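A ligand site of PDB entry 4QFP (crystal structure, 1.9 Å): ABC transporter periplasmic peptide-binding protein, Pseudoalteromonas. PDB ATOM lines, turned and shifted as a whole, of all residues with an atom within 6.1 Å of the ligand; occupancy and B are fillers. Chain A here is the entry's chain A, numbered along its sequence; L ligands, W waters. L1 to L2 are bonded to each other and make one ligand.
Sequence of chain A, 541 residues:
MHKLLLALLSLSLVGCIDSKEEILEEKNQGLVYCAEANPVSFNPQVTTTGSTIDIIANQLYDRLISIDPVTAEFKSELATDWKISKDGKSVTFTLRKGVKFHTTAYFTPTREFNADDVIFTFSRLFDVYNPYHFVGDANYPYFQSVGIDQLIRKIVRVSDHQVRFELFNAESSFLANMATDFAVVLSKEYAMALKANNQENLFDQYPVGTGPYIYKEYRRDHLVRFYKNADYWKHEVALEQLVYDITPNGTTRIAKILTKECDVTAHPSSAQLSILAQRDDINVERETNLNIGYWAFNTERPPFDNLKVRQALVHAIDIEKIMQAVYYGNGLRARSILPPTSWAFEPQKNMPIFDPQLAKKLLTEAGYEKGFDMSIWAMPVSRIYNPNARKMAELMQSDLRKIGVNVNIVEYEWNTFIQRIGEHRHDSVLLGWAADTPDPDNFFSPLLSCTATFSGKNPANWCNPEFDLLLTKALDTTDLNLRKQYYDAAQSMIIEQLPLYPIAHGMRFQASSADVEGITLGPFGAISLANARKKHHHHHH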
ATOM      1  N   THR A  47      -9.773   5.764  16.356  1.00  0.00           N
ATOM      2  CA  THR A  47     -10.937   6.506  16.847  1.00  0.00           C
ATOM      3  C   THR A  47     -11.693   5.805  17.977  1.00  0.00           C
ATOM      4  O   THR A  47     -11.635   4.592  18.133  1.00  0.00           O
ATOM      5  CB  THR A  47     -11.940   6.782  15.721  1.00  0.00           C
ATOM      6  OG1 THR A  47     -12.992   7.628  16.188  1.00  0.00           O
ATOM      7  CG2 THR A  47     -12.517   5.474  15.210  1.00  0.00           C
ATOM      8  N   THR A  48     -12.421   6.592  18.761  1.00  0.00           N
ATOM      9  CA  THR A  48     -13.327   6.027  19.741  1.00  0.00           C
ATOM     10  C   THR A  48     -14.761   6.459  19.486  1.00  0.00           C
ATOM     11  O   THR A  48     -15.624   6.272  20.328  1.00  0.00           O
ATOM     12  CB  THR A  48     -12.901   6.373  21.183  1.00  0.00           C
ATOM     13  OG1 THR A  48     -12.879   7.795  21.361  1.00  0.00           O
ATOM     14  CG2 THR A  48     -11.521   5.808  21.470  1.00  0.00           C
ATOM     15  N   THR A  49     -15.007   7.043  18.320  1.00  0.00           N
ATOM     16  CA  THR A  49     -16.334   7.562  17.998  1.00  0.00           C
ATOM     17  C   THR A  49     -17.228   6.453  17.465  1.00  0.00           C
ATOM     18  O   THR A  49     -16.925   5.847  16.429  1.00  0.00           O
ATOM     19  CB  THR A  49     -16.266   8.678  16.948  1.00  0.00           C
ATOM     20  OG1 THR A  49     -15.324   9.677  17.354  1.00  0.00           O
ATOM     21  CG2 THR A  49     -17.649   9.316  16.795  1.00  0.00           C
ATOM     22  N   GLY A  50     -18.331   6.210  18.155  1.00  0.00           N
ATOM     23  CA  GLY A  50     -19.191   5.083  17.819  1.00  0.00           C
ATOM     24  C   GLY A  50     -19.696   5.130  16.394  1.00  0.00           C
ATOM     25  O   GLY A  50     -19.948   4.084  15.785  1.00  0.00           O
ATOM     26  N   SER A  51     -19.860   6.346  15.878  1.00  0.00           N
ATOM     27  CA  SER A  51     -20.340   6.550  14.501  1.00  0.00           C
ATOM     28  C   SER A  51     -19.429   5.905  13.472  1.00  0.00           C
ATOM     29  O   SER A  51     -19.880   5.361  12.456  1.00  0.00           O
ATOM     30  CB  SER A  51     -20.417   8.057  14.186  1.00  0.00           C
ATOM     31  OG  SER A  51     -21.299   8.728  15.061  1.00  0.00           O
ATOM     32  N   ILE A  53     -16.970   3.504  14.251  1.00  0.00           N
ATOM     33  CA  ILE A  53     -16.863   2.079  14.593  1.00  0.00           C
ATOM     34  C   ILE A  53     -18.069   1.276  14.115  1.00  0.00           C
ATOM     35  O   ILE A  53     -17.906   0.175  13.584  1.00  0.00           O
ATOM     36  CB  ILE A  53     -16.662   1.879  16.108  1.00  0.00           C
ATOM     37  CG1 ILE A  53     -15.388   2.598  16.574  1.00  0.00           C
ATOM     38  CG2 ILE A  53     -16.590   0.401  16.459  1.00  0.00           C
ATOM     39  CD1 ILE A  53     -14.112   2.050  15.979  1.00  0.00           C
ATOM     40  N   PHE A 182     -11.995  -2.114  18.610  1.00  0.00           N
ATOM     41  CA  PHE A 182     -10.781  -1.415  18.203  1.00  0.00           C
ATOM     42  C   PHE A 182      -9.659  -2.405  17.919  1.00  0.00           C
ATOM     43  O   PHE A 182      -8.652  -2.049  17.271  1.00  0.00           O
ATOM     44  CB  PHE A 182     -10.279  -0.496  19.325  1.00  0.00           C
ATOM     45  CG  PHE A 182     -11.340   0.361  19.939  1.00  0.00           C
ATOM     46  CD1 PHE A 182     -11.943   1.369  19.209  1.00  0.00           C
ATOM     47  CD2 PHE A 182     -11.729   0.148  21.252  1.00  0.00           C
ATOM     48  CE1 PHE A 182     -12.938   2.155  19.782  1.00  0.00           C
ATOM     49  CE2 PHE A 182     -12.714   0.930  21.832  1.00  0.00           C
ATOM     50  CZ  PHE A 182     -13.317   1.939  21.092  1.00  0.00           C
ATOM     51  N   TYR A 294     -23.476  12.101  30.635  1.00  0.00           N
ATOM     52  CA  TYR A 294     -23.018  12.918  31.750  1.00  0.00           C
ATOM     53  C   TYR A 294     -22.814  14.373  31.371  1.00  0.00           C
ATOM     54  O   TYR A 294     -22.850  14.754  30.182  1.00  0.00           O
ATOM     55  CB  TYR A 294     -21.713  12.363  32.327  1.00  0.00           C
ATOM     56  CG  TYR A 294     -20.604  12.223  31.305  1.00  0.00           C
ATOM     57  CD1 TYR A 294     -19.952  13.344  30.805  1.00  0.00           C
ATOM     58  CD2 TYR A 294     -20.184  10.968  30.853  1.00  0.00           C
ATOM     59  CE1 TYR A 294     -18.935  13.225  29.874  1.00  0.00           C
ATOM     60  CE2 TYR A 294     -19.153  10.855  29.931  1.00  0.00           C
ATOM     61  CZ  TYR A 294     -18.538  11.987  29.438  1.00  0.00           C
ATOM     62  OH  TYR A 294     -17.513  11.887  28.518  1.00  0.00           O
ATOM     63  N   MET A 379     -23.842  17.858  21.894  1.00  0.00           N
ATOM     64  CA  MET A 379     -23.734  17.022  20.713  1.00  0.00           C
ATOM     65  C   MET A 379     -24.886  17.289  19.754  1.00  0.00           C
ATOM     66  O   MET A 379     -26.036  17.465  20.162  1.00  0.00           O
ATOM     67  CB  MET A 379     -23.754  15.546  21.131  1.00  0.00           C
ATOM     68  CG  MET A 379     -22.935  15.288  22.372  1.00  0.00           C
ATOM     69  SD  MET A 379     -23.042  13.588  22.905  1.00  0.00           S
ATOM     70  CE  MET A 379     -24.584  13.633  23.831  1.00  0.00           C
ATOM     71  N   ARG A 383     -27.370  10.012  20.582  1.00  0.00           N
ATOM     72  CA  ARG A 383     -26.483   8.937  21.040  1.00  0.00           C
ATOM     73  C   ARG A 383     -27.274   8.044  21.974  1.00  0.00           C
ATOM     74  O   ARG A 383     -28.281   8.475  22.549  1.00  0.00           O
ATOM     75  CB  ARG A 383     -25.277   9.471  21.808  1.00  0.00           C
ATOM     76  CG  ARG A 383     -24.545  10.662  21.181  1.00  0.00           C
ATOM     77  CD  ARG A 383     -24.126  10.379  19.762  1.00  0.00           C
ATOM     78  NE  ARG A 383     -23.057   9.381  19.649  1.00  0.00           N
ATOM     79  CZ  ARG A 383     -23.038   8.435  18.713  1.00  0.00           C
ATOM     80  NH1 ARG A 383     -24.035   8.350  17.832  1.00  0.00           N
ATOM     81  NH2 ARG A 383     -22.023   7.576  18.649  1.00  0.00           N
ATOM     82  N   ILE A 384     -26.803   6.819  22.183  1.00  0.00           N
ATOM     83  CA  ILE A 384     -27.496   5.880  23.044  1.00  0.00           C
ATOM     84  C   ILE A 384     -27.733   6.520  24.402  1.00  0.00           C
ATOM     85  O   ILE A 384     -28.803   6.392  24.980  1.00  0.00           O
ATOM     86  CB  ILE A 384     -26.700   4.584  23.230  1.00  0.00           C
ATOM     87  CG1 ILE A 384     -26.570   3.848  21.907  1.00  0.00           C
ATOM     88  CG2 ILE A 384     -27.370   3.694  24.279  1.00  0.00           C
ATOM     89  CD1 ILE A 384     -25.330   2.971  21.824  1.00  0.00           C
ATOM     90  N   TYR A 385     -26.741   7.255  24.875  1.00  0.00           N
ATOM     91  CA  TYR A 385     -26.735   7.786  26.229  1.00  0.00           C
ATOM     92  C   TYR A 385     -27.331   9.192  26.333  1.00  0.00           C
ATOM     93  O   TYR A 385     -27.473   9.731  27.425  1.00  0.00           O
ATOM     94  CB  TYR A 385     -25.296   7.782  26.749  1.00  0.00           C
ATOM     95  CG  TYR A 385     -24.297   8.420  25.805  1.00  0.00           C
ATOM     96  CD1 TYR A 385     -24.238   9.806  25.655  1.00  0.00           C
ATOM     97  CD2 TYR A 385     -23.397   7.636  25.075  1.00  0.00           C
ATOM     98  CE1 TYR A 385     -23.321  10.399  24.790  1.00  0.00           C
ATOM     99  CE2 TYR A 385     -22.469   8.225  24.218  1.00  0.00           C
ATOM    100  CZ  TYR A 385     -22.444   9.601  24.072  1.00  0.00           C
ATOM    101  OH  TYR A 385     -21.529  10.184  23.216  1.00  0.00           O
ATOM    102  N   TRP A 414     -20.662  16.632  14.217  1.00  0.00           N
ATOM    103  CA  TRP A 414     -20.284  15.640  15.232  1.00  0.00           C
ATOM    104  C   TRP A 414     -18.780  15.337  15.320  1.00  0.00           C
ATOM    105  O   TRP A 414     -18.202  15.369  16.416  1.00  0.00           O
ATOM    106  CB  TRP A 414     -21.103  14.364  15.001  1.00  0.00           C
ATOM    107  CG  TRP A 414     -20.825  13.181  15.913  1.00  0.00           C
ATOM    108  CD1 TRP A 414     -20.575  11.904  15.495  1.00  0.00           C
ATOM    109  CD2 TRP A 414     -20.827  13.138  17.350  1.00  0.00           C
ATOM    110  NE1 TRP A 414     -20.410  11.080  16.569  1.00  0.00           N
ATOM    111  CE2 TRP A 414     -20.561  11.796  17.719  1.00  0.00           C
ATOM    112  CE3 TRP A 414     -21.012  14.088  18.354  1.00  0.00           C
ATOM    113  CZ2 TRP A 414     -20.469  11.394  19.059  1.00  0.00           C
ATOM    114  CZ3 TRP A 414     -20.934  13.681  19.686  1.00  0.00           C
ATOM    115  CH2 TRP A 414     -20.663  12.340  20.024  1.00  0.00           C
ATOM    116  N   ILE A 418     -16.237  16.361  18.424  1.00  0.00           N
ATOM    117  CA  ILE A 418     -15.333  15.478  19.142  1.00  0.00           C
ATOM    118  C   ILE A 418     -13.905  16.022  19.118  1.00  0.00           C
ATOM    119  O   ILE A 418     -13.219  16.049  20.124  1.00  0.00           O
ATOM    120  CB  ILE A 418     -15.386  14.061  18.550  1.00  0.00           C
ATOM    121  CG1 ILE A 418     -16.743  13.417  18.856  1.00  0.00           C
ATOM    122  CG2 ILE A 418     -14.248  13.205  19.071  1.00  0.00           C
ATOM    123  CD1 ILE A 418     -17.011  13.245  20.329  1.00  0.00           C
ATOM    124  N   LEU A 431     -21.727  14.794  27.220  1.00  0.00           N
ATOM    125  CA  LEU A 431     -21.151  13.695  26.467  1.00  0.00           C
ATOM    126  C   LEU A 431     -21.517  12.382  27.139  1.00  0.00           C
ATOM    127  O   LEU A 431     -22.495  12.304  27.882  1.00  0.00           O
ATOM    128  CB  LEU A 431     -19.625  13.833  26.379  1.00  0.00           C
ATOM    129  CG  LEU A 431     -18.990  14.088  25.011  1.00  0.00           C
ATOM    130  CD1 LEU A 431     -17.475  14.066  25.107  1.00  0.00           C
ATOM    131  CD2 LEU A 431     -19.463  13.067  23.972  1.00  0.00           C
ATOM    132  N   GLY A 432     -20.757  11.337  26.886  1.00  0.00           N
ATOM    133  CA  GLY A 432     -21.039  10.055  27.508  1.00  0.00           C
ATOM    134  C   GLY A 432     -20.224   8.939  26.908  1.00  0.00           C
ATOM    135  O   GLY A 432     -19.346   9.174  26.070  1.00  0.00           O
ATOM    136  N   TRP A 433     -20.518   7.720  27.325  1.00  0.00           N
ATOM    137  CA  TRP A 433     -19.747   6.582  26.904  1.00  0.00           C
ATOM    138  C   TRP A 433     -20.654   5.367  26.778  1.00  0.00           C
ATOM    139  O   TRP A 433     -21.342   5.008  27.731  1.00  0.00           O
ATOM    140  CB  TRP A 433     -18.633   6.333  27.913  1.00  0.00           C
ATOM    141  CG  TRP A 433     -17.664   5.253  27.539  1.00  0.00           C
ATOM    142  CD1 TRP A 433     -17.618   4.002  28.049  1.00  0.00           C
ATOM    143  CD2 TRP A 433     -16.582   5.346  26.607  1.00  0.00           C
ATOM    144  NE1 TRP A 433     -16.584   3.296  27.492  1.00  0.00           N
ATOM    145  CE2 TRP A 433     -15.928   4.103  26.598  1.00  0.00           C
ATOM    146  CE3 TRP A 433     -16.115   6.367  25.774  1.00  0.00           C
ATOM    147  CZ2 TRP A 433     -14.828   3.852  25.798  1.00  0.00           C
ATOM    148  CZ3 TRP A 433     -15.018   6.106  24.973  1.00  0.00           C
ATOM    149  CH2 TRP A 433     -14.393   4.860  24.980  1.00  0.00           C
ATOM    150  N   ALA A 434     -20.667   4.759  25.599  1.00  0.00           N
ATOM    151  CA  ALA A 434     -21.342   3.476  25.405  1.00  0.00           C
ATOM    152  C   ALA A 434     -20.292   2.388  25.538  1.00  0.00           C
ATOM    153  O   ALA A 434     -19.395   2.268  24.698  1.00  0.00           O
ATOM    154  CB  ALA A 434     -22.000   3.429  24.053  1.00  0.00           C
ATOM    155  N   ALA A 435     -20.387   1.596  26.597  1.00  0.00           N
ATOM    156  CA  ALA A 435     -19.335   0.627  26.921  1.00  0.00           C
ATOM    157  C   ALA A 435     -19.045  -0.334  25.775  1.00  0.00           C
ATOM    158  O   ALA A 435     -19.948  -0.792  25.070  1.00  0.00           O
ATOM    159  CB  ALA A 435     -19.679  -0.144  28.188  1.00  0.00           C
ATOM    160  N   ASP A 436     -17.761  -0.640  25.632  1.00  0.00           N
ATOM    161  CA  ASP A 436     -17.249  -1.490  24.568  1.00  0.00           C
ATOM    162  C   ASP A 436     -17.224  -2.978  24.966  1.00  0.00           C
ATOM    163  O   ASP A 436     -17.213  -3.853  24.093  1.00  0.00           O
ATOM    164  CB  ASP A 436     -15.831  -1.017  24.187  1.00  0.00           C
ATOM    165  CG  ASP A 436     -15.758   0.497  23.970  1.00  0.00           C
ATOM    166  OD1 ASP A 436     -16.494   1.011  23.110  1.00  0.00           O
ATOM    167  OD2 ASP A 436     -14.978   1.173  24.685  1.00  0.00           O
ATOM    168  N   ASN A 442     -13.736  -0.481  31.542  1.00  0.00           N
ATOM    169  CA  ASN A 442     -14.057   0.248  30.317  1.00  0.00           C
ATOM    170  C   ASN A 442     -14.753   1.610  30.564  1.00  0.00           C
ATOM    171  O   ASN A 442     -14.665   2.511  29.726  1.00  0.00           O
ATOM    172  CB  ASN A 442     -14.867  -0.651  29.371  1.00  0.00           C
ATOM    173  CG  ASN A 442     -15.095  -0.044  28.001  1.00  0.00           C
ATOM    174  OD1 ASN A 442     -14.190   0.003  27.162  1.00  0.00           O
ATOM    175  ND2 ASN A 442     -16.318   0.383  27.751  1.00  0.00           N
ATOM    176  N   GLY A 525     -20.713  -2.691  22.879  1.00  0.00           N
ATOM    177  CA  GLY A 525     -20.014  -2.825  21.620  1.00  0.00           C
ATOM    178  C   GLY A 525     -20.777  -2.304  20.417  1.00  0.00           C
ATOM    179  O   GLY A 525     -21.858  -1.746  20.552  1.00  0.00           O
HETATM  180  N1  LIG L   1     -17.098   3.530  23.292  1.00  0.00           N
HETATM  181  C1  LIG L   1     -17.130   4.600  22.292  1.00  0.00           C
HETATM  182  C2  LIG L   1     -18.049   5.732  22.727  1.00  0.00           C
HETATM  183  O1  LIG L   1     -18.835   5.597  23.656  1.00  0.00           O
HETATM  184  C3  LIG L   1     -17.657   4.099  20.947  1.00  0.00           C
HETATM  185  C4  LIG L   1     -16.739   3.045  20.339  1.00  0.00           C
HETATM  186  C5  LIG L   1     -19.075   3.560  21.114  1.00  0.00           C
HETATM  187  N1  LG2 L   2     -17.958   6.862  22.024  1.00  0.00           N
HETATM  188  C1  LG2 L   2     -18.864   7.978  22.239  1.00  0.00           C
HETATM  189  C2  LG2 L   2     -20.058   7.858  21.283  1.00  0.00           C
HETATM  190  O1  LG2 L   2     -21.080   8.556  21.397  1.00  0.00           O
HETATM  191  C3  LG2 L   2     -18.163   9.323  22.008  1.00  0.00           C
HETATM  192  O2  LG2 L   2     -17.518   9.303  20.732  1.00  0.00           O
HETATM  193  C4  LG2 L   2     -17.116   9.575  23.089  1.00  0.00           C
HETATM  194  O3  LG2 L   2     -20.006   7.060  20.342  1.00  0.00           O
HETATM  195  O   HOH W   1     -20.176   1.866  18.547  1.00  0.00           O
HETATM  196  O   HOH W   2     -18.380   0.159  19.380  1.00  0.00           O
HETATM  197  O   HOH W   3     -22.116   2.365  20.073  1.00  0.00           O
HETATM  198  O   HOH W   4     -14.824   9.669  20.495  1.00  0.00           O
HETATM  199  O   HOH W   5     -22.303   4.898  20.136  1.00  0.00           O
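OH of Tyr 385 lies within hydrogen-bond range of O1 of LG2 L2 (2.5 Å).
The side-chain carboxylate (OD1) of Asp 436 is in salt-bridge range of a nitrogen (N1) of LIG L1.
NH2 of Arg 383 is in salt-bridge range of O3 of LG2 L2, 2.7 Å away.
N of Ala 434 is in hydrogen-bond range of O1 of LIG L1, at 2.8 Å.
N1 of LIG L1 is in hydrogen-bond range of O of Ala 434, 3.0 Å away.
N of Gly 50 lies within hydrogen-bond range of O3 of LG2 L2 (2.9 Å).
N1 of LG2 L2 sits at hydrogen-bond distance from O of Thr 48.
The side-chain sulfur (SD) of Met 379 lies close to the side-chain hydroxyl (OH) of Tyr 385, at 3.7 Å.
ND2 of Asn 442 lies close to N of Asp 436.
The indole nitrogen (NE1) of Trp 433 sits close to the side-chain amide nitrogen (ND2) of Asn 442, 2.9 Å away.
The backbone NH of Thr 49 lies within hydrogen-bond range of the side-chain hydroxyl of Thr 47 (3.0 Å).
The indole nitrogen (NE1) of Trp 414 lies within hydrogen-bond range of the side-chain hydroxyl (OG) of Ser 51 (2.9 Å).
Residues that only touch the ligand: Thr 49, Phe 182, Trp 414, Ile 418, Gly 432 and Trp 433.
Hydrophobic or aromatic side chains within 4 Å of the ligand: Phe 182, Tyr 385, Trp 414, Ile 418, Trp 433 and Ala 434.
12 residues have an atom within 4 Å of the ligand: Thr 48, Thr 49, Gly 50, Phe 182, Arg 383, Tyr 385, Trp 414, Ile 418, Gly 432, Trp 433, Ala 434 and Asp 436.
Water W4 lies within hydrogen-bond range of O2 of LG2 L2, OG1 of Thr 48 and OG1 of Thr 49.
Water W5 lies within hydrogen-bond range of the guanidinium group (NH2) of Arg 383 (3.1 Å) and an oxygen (O3) of LG2 L2 (3.2 Å).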
